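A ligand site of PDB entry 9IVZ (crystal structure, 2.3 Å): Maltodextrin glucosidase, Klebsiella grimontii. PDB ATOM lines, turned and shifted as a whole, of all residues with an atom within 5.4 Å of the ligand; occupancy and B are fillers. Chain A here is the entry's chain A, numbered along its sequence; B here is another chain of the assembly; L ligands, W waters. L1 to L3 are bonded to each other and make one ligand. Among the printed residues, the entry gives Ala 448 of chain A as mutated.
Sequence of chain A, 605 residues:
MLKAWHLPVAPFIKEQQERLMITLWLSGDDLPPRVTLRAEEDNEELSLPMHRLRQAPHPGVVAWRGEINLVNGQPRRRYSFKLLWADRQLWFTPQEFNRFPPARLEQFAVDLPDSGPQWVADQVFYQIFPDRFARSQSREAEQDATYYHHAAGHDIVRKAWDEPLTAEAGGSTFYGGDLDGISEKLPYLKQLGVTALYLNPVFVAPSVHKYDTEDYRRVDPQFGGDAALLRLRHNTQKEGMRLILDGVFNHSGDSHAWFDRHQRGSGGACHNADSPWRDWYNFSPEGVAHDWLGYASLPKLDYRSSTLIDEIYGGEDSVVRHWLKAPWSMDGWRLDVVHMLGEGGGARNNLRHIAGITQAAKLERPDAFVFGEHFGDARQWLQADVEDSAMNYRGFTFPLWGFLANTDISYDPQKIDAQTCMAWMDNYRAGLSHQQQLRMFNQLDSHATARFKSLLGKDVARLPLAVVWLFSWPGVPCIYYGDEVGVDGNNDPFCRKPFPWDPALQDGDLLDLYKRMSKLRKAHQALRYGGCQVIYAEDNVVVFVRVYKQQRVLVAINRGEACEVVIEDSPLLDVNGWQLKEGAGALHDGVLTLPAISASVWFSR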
ATOM      1  N   GLY A 170       9.500  28.364  26.923  1.00  0.00           N
ATOM      2  CA  GLY A 170       8.377  27.443  26.817  1.00  0.00           C
ATOM      3  C   GLY A 170       8.340  26.632  25.532  1.00  0.00           C
ATOM      4  O   GLY A 170       7.784  25.538  25.505  1.00  0.00           O
ATOM      5  N   GLY A 171       8.929  27.142  24.462  1.00  0.00           N
ATOM      6  CA  GLY A 171       8.959  26.440  23.201  1.00  0.00           C
ATOM      7  C   GLY A 171      10.231  25.698  22.928  1.00  0.00           C
ATOM      8  O   GLY A 171      10.338  25.046  21.876  1.00  0.00           O
ATOM      9  N   VAL A 208       9.928  22.597  20.553  1.00  0.00           N
ATOM     10  CA  VAL A 208       9.465  21.375  21.214  1.00  0.00           C
ATOM     11  C   VAL A 208       8.073  20.999  20.732  1.00  0.00           C
ATOM     12  O   VAL A 208       7.735  19.809  20.685  1.00  0.00           O
ATOM     13  CB  VAL A 208       9.503  21.548  22.739  1.00  0.00           C
ATOM     14  CG1 VAL A 208       8.527  22.652  23.189  1.00  0.00           C
ATOM     15  CG2 VAL A 208       9.179  20.238  23.440  1.00  0.00           C
ATOM     16  N   HIS A 209       7.237  21.967  20.362  1.00  0.00           N
ATOM     17  CA  HIS A 209       5.891  21.661  19.896  1.00  0.00           C
ATOM     18  C   HIS A 209       5.852  21.339  18.410  1.00  0.00           C
ATOM     19  O   HIS A 209       4.984  20.581  17.966  1.00  0.00           O
ATOM     20  CB  HIS A 209       4.971  22.829  20.225  1.00  0.00           C
ATOM     21  CG  HIS A 209       5.466  24.143  19.708  1.00  0.00           C
ATOM     22  ND1 HIS A 209       5.414  24.481  18.367  1.00  0.00           N
ATOM     23  CD2 HIS A 209       6.077  25.168  20.332  1.00  0.00           C
ATOM     24  CE1 HIS A 209       5.963  25.666  18.202  1.00  0.00           C
ATOM     25  NE2 HIS A 209       6.365  26.116  19.377  1.00  0.00           N
ATOM     26  N   TYR A 211       5.160  23.071  15.644  1.00  0.00           N
ATOM     27  CA  TYR A 211       4.298  23.714  14.645  1.00  0.00           C
ATOM     28  C   TYR A 211       5.096  24.623  13.725  1.00  0.00           C
ATOM     29  O   TYR A 211       4.540  25.166  12.763  1.00  0.00           O
ATOM     30  CB  TYR A 211       3.163  24.492  15.322  1.00  0.00           C
ATOM     31  CG  TYR A 211       2.099  23.592  15.911  1.00  0.00           C
ATOM     32  CD1 TYR A 211       1.141  22.991  15.091  1.00  0.00           C
ATOM     33  CD2 TYR A 211       2.063  23.320  17.270  1.00  0.00           C
ATOM     34  CE1 TYR A 211       0.163  22.140  15.623  1.00  0.00           C
ATOM     35  CE2 TYR A 211       1.108  22.455  17.810  1.00  0.00           C
ATOM     36  CZ  TYR A 211       0.166  21.877  16.984  1.00  0.00           C
ATOM     37  OH  TYR A 211      -0.773  21.023  17.544  1.00  0.00           O
ATOM     38  N   VAL A 248       0.059  20.728   9.634  1.00  0.00           N
ATOM     39  CA  VAL A 248       0.322  22.153   9.856  1.00  0.00           C
ATOM     40  C   VAL A 248       0.572  22.842   8.515  1.00  0.00           C
ATOM     41  O   VAL A 248       1.715  23.050   8.121  1.00  0.00           O
ATOM     42  CB  VAL A 248       1.504  22.351  10.816  1.00  0.00           C
ATOM     43  CG1 VAL A 248       1.546  23.801  11.339  1.00  0.00           C
ATOM     44  CG2 VAL A 248       1.407  21.353  11.977  1.00  0.00           C
ATOM     45  N   HIS A 251       0.905  27.496   7.640  1.00  0.00           N
ATOM     46  CA  HIS A 251       2.153  28.209   7.792  1.00  0.00           C
ATOM     47  C   HIS A 251       3.265  27.178   7.936  1.00  0.00           C
ATOM     48  O   HIS A 251       3.020  26.059   8.380  1.00  0.00           O
ATOM     49  CB  HIS A 251       2.100  29.121   9.019  1.00  0.00           C
ATOM     50  CG  HIS A 251       1.973  28.357  10.298  1.00  0.00           C
ATOM     51  ND1 HIS A 251       0.780  28.199  10.967  1.00  0.00           N
ATOM     52  CD2 HIS A 251       2.891  27.650  11.007  1.00  0.00           C
ATOM     53  CE1 HIS A 251       0.969  27.466  12.047  1.00  0.00           C
ATOM     54  NE2 HIS A 251       2.246  27.113  12.089  1.00  0.00           N
ATOM     55  N   TRP A 292       3.731  36.637  10.406  1.00  0.00           N
ATOM     56  CA  TRP A 292       2.333  36.206  10.477  1.00  0.00           C
ATOM     57  C   TRP A 292       1.845  36.422  11.900  1.00  0.00           C
ATOM     58  O   TRP A 292       2.438  35.904  12.848  1.00  0.00           O
ATOM     59  CB  TRP A 292       2.143  34.746  10.064  1.00  0.00           C
ATOM     60  CG  TRP A 292       0.693  34.340  10.203  1.00  0.00           C
ATOM     61  CD1 TRP A 292      -0.388  34.953   9.620  1.00  0.00           C
ATOM     62  CD2 TRP A 292       0.160  33.255  10.977  1.00  0.00           C
ATOM     63  NE1 TRP A 292      -1.558  34.322   9.996  1.00  0.00           N
ATOM     64  CE2 TRP A 292      -1.250  33.277  10.816  1.00  0.00           C
ATOM     65  CE3 TRP A 292       0.725  32.256  11.787  1.00  0.00           C
ATOM     66  CZ2 TRP A 292      -2.082  32.338  11.442  1.00  0.00           C
ATOM     67  CZ3 TRP A 292      -0.102  31.344  12.395  1.00  0.00           C
ATOM     68  CH2 TRP A 292      -1.495  31.386  12.218  1.00  0.00           C
ATOM     69  N   LEU A 293       0.749  37.157  12.031  1.00  0.00           N
ATOM     70  CA  LEU A 293       0.286  37.619  13.341  1.00  0.00           C
ATOM     71  C   LEU A 293       1.494  38.185  14.083  1.00  0.00           C
ATOM     72  O   LEU A 293       2.176  39.071  13.569  1.00  0.00           O
ATOM     73  CB  LEU A 293      -0.393  36.498  14.127  1.00  0.00           C
ATOM     74  CG  LEU A 293      -1.653  35.913  13.449  1.00  0.00           C
ATOM     75  CD1 LEU A 293      -2.497  35.102  14.425  1.00  0.00           C
ATOM     76  CD2 LEU A 293      -2.504  36.962  12.751  1.00  0.00           C
ATOM     77  N   TYR A 295       4.204  36.398  14.764  1.00  0.00           N
ATOM     78  CA  TYR A 295       5.247  35.375  14.702  1.00  0.00           C
ATOM     79  C   TYR A 295       6.183  35.601  13.535  1.00  0.00           C
ATOM     80  O   TYR A 295       5.775  35.500  12.367  1.00  0.00           O
ATOM     81  CB  TYR A 295       4.620  33.983  14.586  1.00  0.00           C
ATOM     82  CG  TYR A 295       3.671  33.645  15.693  1.00  0.00           C
ATOM     83  CD1 TYR A 295       4.154  33.332  16.960  1.00  0.00           C
ATOM     84  CD2 TYR A 295       2.297  33.618  15.468  1.00  0.00           C
ATOM     85  CE1 TYR A 295       3.293  32.995  17.995  1.00  0.00           C
ATOM     86  CE2 TYR A 295       1.424  33.288  16.499  1.00  0.00           C
ATOM     87  CZ  TYR A 295       1.927  32.980  17.768  1.00  0.00           C
ATOM     88  OH  TYR A 295       1.085  32.647  18.804  1.00  0.00           O
ATOM     89  N   SER A 297       8.512  33.341  13.553  1.00  0.00           N
ATOM     90  CA  SER A 297       8.868  31.934  13.373  1.00  0.00           C
ATOM     91  C   SER A 297       7.899  31.173  12.478  1.00  0.00           C
ATOM     92  O   SER A 297       8.264  30.098  11.993  1.00  0.00           O
ATOM     93  CB  SER A 297       8.968  31.232  14.728  1.00  0.00           C
ATOM     94  OG  SER A 297       7.761  31.350  15.449  1.00  0.00           O
ATOM     95  N   LEU A 298       6.693  31.684  12.242  1.00  0.00           N
ATOM     96  CA  LEU A 298       5.624  30.928  11.587  1.00  0.00           C
ATOM     97  C   LEU A 298       5.080  31.643  10.354  1.00  0.00           C
ATOM     98  O   LEU A 298       3.887  31.949  10.287  1.00  0.00           O
ATOM     99  CB  LEU A 298       4.490  30.636  12.566  1.00  0.00           C
ATOM    100  CG  LEU A 298       4.809  30.011  13.926  1.00  0.00           C
ATOM    101  CD1 LEU A 298       3.620  30.033  14.844  1.00  0.00           C
ATOM    102  CD2 LEU A 298       5.303  28.585  13.741  1.00  0.00           C
ATOM    103  N   ASP A 336      -4.187  21.838  11.586  1.00  0.00           N
ATOM    104  CA  ASP A 336      -3.873  22.969  12.450  1.00  0.00           C
ATOM    105  C   ASP A 336      -4.248  24.279  11.764  1.00  0.00           C
ATOM    106  O   ASP A 336      -4.087  24.401  10.550  1.00  0.00           O
ATOM    107  CB  ASP A 336      -2.386  22.963  12.788  1.00  0.00           C
ATOM    108  CG  ASP A 336      -1.986  24.102  13.716  1.00  0.00           C
ATOM    109  OD1 ASP A 336      -2.545  24.187  14.821  1.00  0.00           O
ATOM    110  OD2 ASP A 336      -1.111  24.905  13.345  1.00  0.00           O
ATOM    111  N   VAL A 337      -4.744  25.242  12.545  1.00  0.00           N
ATOM    112  CA  VAL A 337      -5.195  26.554  12.050  1.00  0.00           C
ATOM    113  C   VAL A 337      -6.022  26.380  10.793  1.00  0.00           C
ATOM    114  O   VAL A 337      -5.736  26.995   9.759  1.00  0.00           O
ATOM    115  CB  VAL A 337      -3.990  27.498  11.797  1.00  0.00           C
ATOM    116  CG1 VAL A 337      -4.466  28.947  11.657  1.00  0.00           C
ATOM    117  CG2 VAL A 337      -2.956  27.392  12.893  1.00  0.00           C
ATOM    118  N   HIS A 339      -8.971  27.295   9.992  1.00  0.00           N
ATOM    119  CA  HIS A 339      -9.859  28.395   9.655  1.00  0.00           C
ATOM    120  C   HIS A 339      -9.139  29.601   9.048  1.00  0.00           C
ATOM    121  O   HIS A 339      -9.807  30.505   8.533  1.00  0.00           O
ATOM    122  CB  HIS A 339     -10.609  28.825  10.913  1.00  0.00           C
ATOM    123  CG  HIS A 339      -9.709  29.378  11.987  1.00  0.00           C
ATOM    124  ND1 HIS A 339      -8.568  28.728  12.409  1.00  0.00           N
ATOM    125  CD2 HIS A 339      -9.779  30.530  12.702  1.00  0.00           C
ATOM    126  CE1 HIS A 339      -7.984  29.451  13.347  1.00  0.00           C
ATOM    127  NE2 HIS A 339      -8.692  30.545  13.540  1.00  0.00           N
ATOM    128  N   MET A 340      -7.812  29.664   9.104  1.00  0.00           N
ATOM    129  CA  MET A 340      -7.103  30.836   8.614  1.00  0.00           C
ATOM    130  C   MET A 340      -6.277  30.566   7.366  1.00  0.00           C
ATOM    131  O   MET A 340      -5.857  31.520   6.706  1.00  0.00           O
ATOM    132  CB  MET A 340      -6.200  31.417   9.701  1.00  0.00           C
ATOM    133  CG  MET A 340      -6.953  31.765  10.976  1.00  0.00           C
ATOM    134  SD  MET A 340      -5.941  32.534  12.248  1.00  0.00           S
ATOM    135  CE  MET A 340      -5.790  34.193  11.584  1.00  0.00           C
ATOM    136  N   GLU A 373      -8.931  22.082  13.718  1.00  0.00           N
ATOM    137  CA  GLU A 373      -9.012  22.725  15.022  1.00  0.00           C
ATOM    138  C   GLU A 373      -9.840  24.000  14.890  1.00  0.00           C
ATOM    139  O   GLU A 373      -9.404  24.968  14.259  1.00  0.00           O
ATOM    140  CB  GLU A 373      -7.621  23.043  15.555  1.00  0.00           C
ATOM    141  CG  GLU A 373      -7.656  23.857  16.829  1.00  0.00           C
ATOM    142  CD  GLU A 373      -6.290  24.422  17.221  1.00  0.00           C
ATOM    143  OE1 GLU A 373      -5.740  25.282  16.473  1.00  0.00           O
ATOM    144  OE2 GLU A 373      -5.776  23.987  18.289  1.00  0.00           O
ATOM    145  N   PHE A 375     -11.398  26.566  17.389  1.00  0.00           N
ATOM    146  CA  PHE A 375     -11.819  27.289  18.594  1.00  0.00           C
ATOM    147  C   PHE A 375     -13.134  28.011  18.367  1.00  0.00           C
ATOM    148  O   PHE A 375     -13.905  28.222  19.312  1.00  0.00           O
ATOM    149  CB  PHE A 375     -10.732  28.270  19.026  1.00  0.00           C
ATOM    150  CG  PHE A 375      -9.660  27.650  19.887  1.00  0.00           C
ATOM    151  CD1 PHE A 375      -8.761  26.734  19.341  1.00  0.00           C
ATOM    152  CD2 PHE A 375      -9.575  27.948  21.228  1.00  0.00           C
ATOM    153  CE1 PHE A 375      -7.770  26.136  20.130  1.00  0.00           C
ATOM    154  CE2 PHE A 375      -8.587  27.357  22.035  1.00  0.00           C
ATOM    155  CZ  PHE A 375      -7.688  26.447  21.476  1.00  0.00           C
ATOM    156  N   HIS A 447      -3.488  20.874  24.145  1.00  0.00           N
ATOM    157  CA  HIS A 447      -2.206  21.553  24.218  1.00  0.00           C
ATOM    158  C   HIS A 447      -2.317  23.067  24.088  1.00  0.00           C
ATOM    159  O   HIS A 447      -1.329  23.767  24.313  1.00  0.00           O
ATOM    160  CB  HIS A 447      -1.294  21.031  23.122  1.00  0.00           C
ATOM    161  CG  HIS A 447      -1.799  21.337  21.758  1.00  0.00           C
ATOM    162  ND1 HIS A 447      -2.936  20.751  21.247  1.00  0.00           N
ATOM    163  CD2 HIS A 447      -1.360  22.208  20.808  1.00  0.00           C
ATOM    164  CE1 HIS A 447      -3.171  21.226  20.025  1.00  0.00           C
ATOM    165  NE2 HIS A 447      -2.228  22.109  19.743  1.00  0.00           N
ATOM    166  N   ALA A 448      -3.491  23.577  23.686  1.00  0.00           N
ATOM    167  CA  ALA A 448      -3.716  24.994  23.445  1.00  0.00           C
ATOM    168  C   ALA A 448      -4.666  25.619  24.457  1.00  0.00           C
ATOM    169  O   ALA A 448      -5.084  26.772  24.277  1.00  0.00           O
ATOM    170  CB  ALA A 448      -4.238  25.210  22.024  1.00  0.00           C
ATOM    171  N   ASP A 492      -0.758  26.860  28.160  1.00  0.00           N
ATOM    172  CA  ASP A 492       0.496  26.861  27.416  1.00  0.00           C
ATOM    173  C   ASP A 492       1.442  27.931  27.957  1.00  0.00           C
ATOM    174  O   ASP A 492       1.141  29.128  27.865  1.00  0.00           O
ATOM    175  CB  ASP A 492       0.159  27.093  25.942  1.00  0.00           C
ATOM    176  CG  ASP A 492       1.358  27.016  25.045  1.00  0.00           C
ATOM    177  OD1 ASP A 492       2.406  26.505  25.482  1.00  0.00           O
ATOM    178  OD2 ASP A 492       1.247  27.472  23.880  1.00  0.00           O
ATOM    179  N   PRO A 493       2.608  27.546  28.495  1.00  0.00           N
ATOM    180  CA  PRO A 493       3.252  26.223  28.478  1.00  0.00           C
ATOM    181  C   PRO A 493       2.800  25.193  29.533  1.00  0.00           C
ATOM    182  O   PRO A 493       3.144  24.020  29.378  1.00  0.00           O
ATOM    183  CB  PRO A 493       4.718  26.581  28.699  1.00  0.00           C
ATOM    184  CG  PRO A 493       4.652  27.737  29.627  1.00  0.00           C
ATOM    185  CD  PRO A 493       3.479  28.556  29.120  1.00  0.00           C
ATOM    186  N   ARG A 496       1.269  21.344  29.294  1.00  0.00           N
ATOM    187  CA  ARG A 496       2.070  20.299  28.660  1.00  0.00           C
ATOM    188  C   ARG A 496       3.041  19.678  29.657  1.00  0.00           C
ATOM    189  O   ARG A 496       4.218  19.467  29.347  1.00  0.00           O
ATOM    190  CB  ARG A 496       2.808  20.873  27.451  1.00  0.00           C
ATOM    191  CG  ARG A 496       1.876  21.549  26.463  1.00  0.00           C
ATOM    192  CD  ARG A 496       2.588  22.521  25.551  1.00  0.00           C
ATOM    193  NE  ARG A 496       1.596  23.221  24.749  1.00  0.00           N
ATOM    194  CZ  ARG A 496       1.856  23.887  23.630  1.00  0.00           C
ATOM    195  NH1 ARG A 496       3.096  24.000  23.165  1.00  0.00           N
ATOM    196  NH2 ARG A 496       0.846  24.438  22.962  1.00  0.00           N
ATOM    197  N   GLU B  44     -10.539  34.270  12.716  1.00  0.00           N
ATOM    198  CA  GLU B  44     -10.114  34.133  14.107  1.00  0.00           C
ATOM    199  C   GLU B  44     -10.921  35.083  14.986  1.00  0.00           C
ATOM    200  O   GLU B  44     -11.097  36.259  14.652  1.00  0.00           O
ATOM    201  CB  GLU B  44      -8.626  34.413  14.251  1.00  0.00           C
ATOM    202  CG  GLU B  44      -8.132  34.502  15.691  1.00  0.00           C
ATOM    203  CD  GLU B  44      -7.958  33.141  16.344  1.00  0.00           C
ATOM    204  OE1 GLU B  44      -8.605  32.176  15.896  1.00  0.00           O
ATOM    205  OE2 GLU B  44      -7.174  33.048  17.313  1.00  0.00           O
HETATM  206  C1  LIG L   1      -6.665  30.007  18.932  1.00  0.00           C
HETATM  207  C2  LIG L   1      -6.417  29.826  17.441  1.00  0.00           C
HETATM  208  C3  LIG L   1      -5.526  28.646  17.123  1.00  0.00           C
HETATM  209  C4  LIG L   1      -4.584  28.206  18.245  1.00  0.00           C
HETATM  210  C5  LIG L   1      -4.605  28.983  19.587  1.00  0.00           C
HETATM  211  C6  LIG L   1      -3.270  29.147  20.229  1.00  0.00           C
HETATM  212  O1  LIG L   1      -7.543  31.107  19.173  1.00  0.00           O
HETATM  213  O2  LIG L   1      -7.686  29.687  16.800  1.00  0.00           O
HETATM  214  O3  LIG L   1      -4.900  28.829  15.828  1.00  0.00           O
HETATM  215  O4  LIG L   1      -3.285  27.583  17.956  1.00  0.00           O
HETATM  216  O5  LIG L   1      -5.372  30.262  19.580  1.00  0.00           O
HETATM  217  O6  LIG L   1      -2.887  30.481  20.201  1.00  0.00           O
HETATM  218  C1  LG2 L   2      -2.289  28.002  17.072  1.00  0.00           C
HETATM  219  C2  LG2 L   2      -1.453  26.755  16.865  1.00  0.00           C
HETATM  220  C3  LG2 L   2      -0.084  26.950  16.349  1.00  0.00           C
HETATM  221  C4  LG2 L   2       0.646  28.091  16.962  1.00  0.00           C
HETATM  222  C5  LG2 L   2      -0.208  29.346  17.110  1.00  0.00           C
HETATM  223  C6  LG2 L   2      -0.454  30.094  15.782  1.00  0.00           C
HETATM  224  O1  LG2 L   2      -1.327  26.008  18.144  1.00  0.00           O
HETATM  225  O2  LG2 L   2      -0.150  27.067  14.890  1.00  0.00           O
HETATM  226  O3  LG2 L   2       1.095  27.706  18.344  1.00  0.00           O
HETATM  227  O4  LG2 L   2      -1.519  29.088  17.721  1.00  0.00           O
HETATM  228  O5  LG2 L   2      -1.263  31.237  16.071  1.00  0.00           O
HETATM  229  O1  LG3 L   3       3.493  27.838  18.139  1.00  0.00           O
HETATM  230  C1  LG3 L   3       2.471  26.400  19.827  1.00  0.00           C
HETATM  231  C2  LG3 L   3       2.595  27.441  20.898  1.00  0.00           C
HETATM  232  C3  LG3 L   3       5.842  28.329  23.152  1.00  0.00           C
HETATM  233  C4  LG3 L   3       6.333  32.535  24.055  1.00  0.00           C
HETATM  234  C5  LG3 L   3       5.650  31.180  23.747  1.00  0.00           C
HETATM  235  C6  LG3 L   3       5.799  30.672  22.214  1.00  0.00           C
HETATM  236  C7  LG3 L   3       5.400  29.346  21.863  1.00  0.00           C
HETATM  237  C8  LG3 L   3       3.173  28.794  20.529  1.00  0.00           C
HETATM  238  C9  LG3 L   3       3.531  29.058  19.007  1.00  0.00           C
HETATM  239  C10 LG3 L   3       4.760  29.830  18.657  1.00  0.00           C
HETATM  240  C11 LG3 L   3       2.328  26.988  18.420  1.00  0.00           C
HETATM  241  C12 LG3 L   3       5.125  28.633  24.202  1.00  0.00           C
HETATM  242  C13 LG3 L   3       5.603  30.180  24.787  1.00  0.00           C
HETATM  243  N1  LG3 L   3       3.960  29.407  21.705  1.00  0.00           N
HETATM  244  O2  LG3 L   3       5.862  33.058  25.301  1.00  0.00           O
HETATM  245  O3  LG3 L   3       1.290  25.666  20.108  1.00  0.00           O
HETATM  246  O4  LG3 L   3       3.203  26.865  22.092  1.00  0.00           O
HETATM  247  O5  LG3 L   3       5.664  26.955  22.732  1.00  0.00           O
HETATM  248  O6  LG3 L   3       5.268  27.689  25.294  1.00  0.00           O
HETATM  249  O7  LG3 L   3       4.722  30.544  25.792  1.00  0.00           O
HETATM  250  O   HOH W   1      -1.100  27.707  22.216  1.00  0.00           O
HETATM  251  O   HOH W   2       5.264  34.794  27.424  1.00  0.00           O
HETATM  252  O   HOH W   3      -2.763  23.918  17.422  1.00  0.00           O
HETATM  253  O   HOH W   4      -3.861  31.020  15.016  1.00  0.00           O
HETATM  254  O   HOH W   5       2.539  31.645  21.411  1.00  0.00           O
HETATM  255  O   HOH W   6      -9.119  27.428  15.710  1.00  0.00           O
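CA of Gly 171 touches O5 of LG3 L3, 3.4 Å away. His 209 touches the ligand. CD2 of Tyr 211 touches O3 of LG3 L3 (3.8 Å). CE1 of His 251 touches O2 of LG2 L2 (3.1 Å). CZ3 of Trp 292 touches C6 of LG2 L2, at 3.6 Å. CE2 of Tyr 295 touches O5 of LG2 L2, 3.4 Å away. CD1 of Leu 298 touches O1 of LG3 L3 (3.96 Å). Val 337 touches the ligand. His 339 touches the ligand. Glu 373 touches the ligand. CD1 of Phe 375 touches C1 of LIG L1 (3.9 Å). Pro 493 touches the ligand. Hydrophobic or aromatic side chains within 4 Å of the ligand: His 209, Tyr 211, His 251, Trp 292, Tyr 295, Leu 298, Val 337, His 339, Phe 375 and Pro 493. Of the 24 residues printed, 17 come within 4 Å of the ligand.
The side-chain carboxylate (OE2) of Glu 44 of chain B sits at hydrogen-bond distance from an oxygen (O1) of LIG L1 (2.7 Å). OD2 of Asp 492 is in salt-bridge range of N1 of LG3 L3, at 3.98 Å. The side-chain carboxylate of Asp 336 lies within hydrogen-bond range of an oxygen (O2) of LG2 L2 (2.8 Å). An oxygen (O4) of LG3 L3 sits at hydrogen-bond distance from the guanidinium group (NH1) of Arg 496 (3.1 Å). An oxygen (O6) of LG3 L3 lies close to the backbone carbonyl oxygen (O) of Gly 170, at 3.3 Å.
A ring nitrogen (NE2) of His 339 is in hydrogen-bond range of the side-chain carboxylate (OE1) of Glu 44 of chain B (2.9 Å). The side-chain carboxylate (OD2) of Asp 492 is in salt-bridge range of the guanidinium group (NH2) of Arg 496. A ring nitrogen (ND1) of His 209 sits at hydrogen-bond distance from the backbone NH (N) of Tyr 211, 3.1 Å away. NH2 of Arg 496 is in hydrogen-bond range of O of His 447, at 2.6 Å. A ring nitrogen (NE2) of His 251 sits at hydrogen-bond distance from the backbone carbonyl oxygen (O) of Tyr 211. O of Gly 171 lies within hydrogen-bond range of N of Val 208 (2.8 Å). NE2 of His 339 sits close to SD of Met 340, 3.6 Å away. The side-chain hydroxyl of Tyr 211 is in hydrogen-bond range of a ring nitrogen (NE2) of His 447 (2.9 Å).
Water W4 bridges an oxygen (O3) of LIG L1 and the side-chain sulfur of Met 340. Water W3 lies within hydrogen-bond range of the side-chain carboxylate of Asp 336, an oxygen (O1) of LG2 L2, a ring nitrogen (NE2) of His 447 and the side-chain carboxylate of Glu 373. Water W5 lies within hydrogen-bond range of a nitrogen (N1) of LG3 L3 and the side-chain hydroxyl of Tyr 295. Water W6 lies within hydrogen-bond range of O of Glu 373, O2 of LIG L1 and N of Phe 375.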
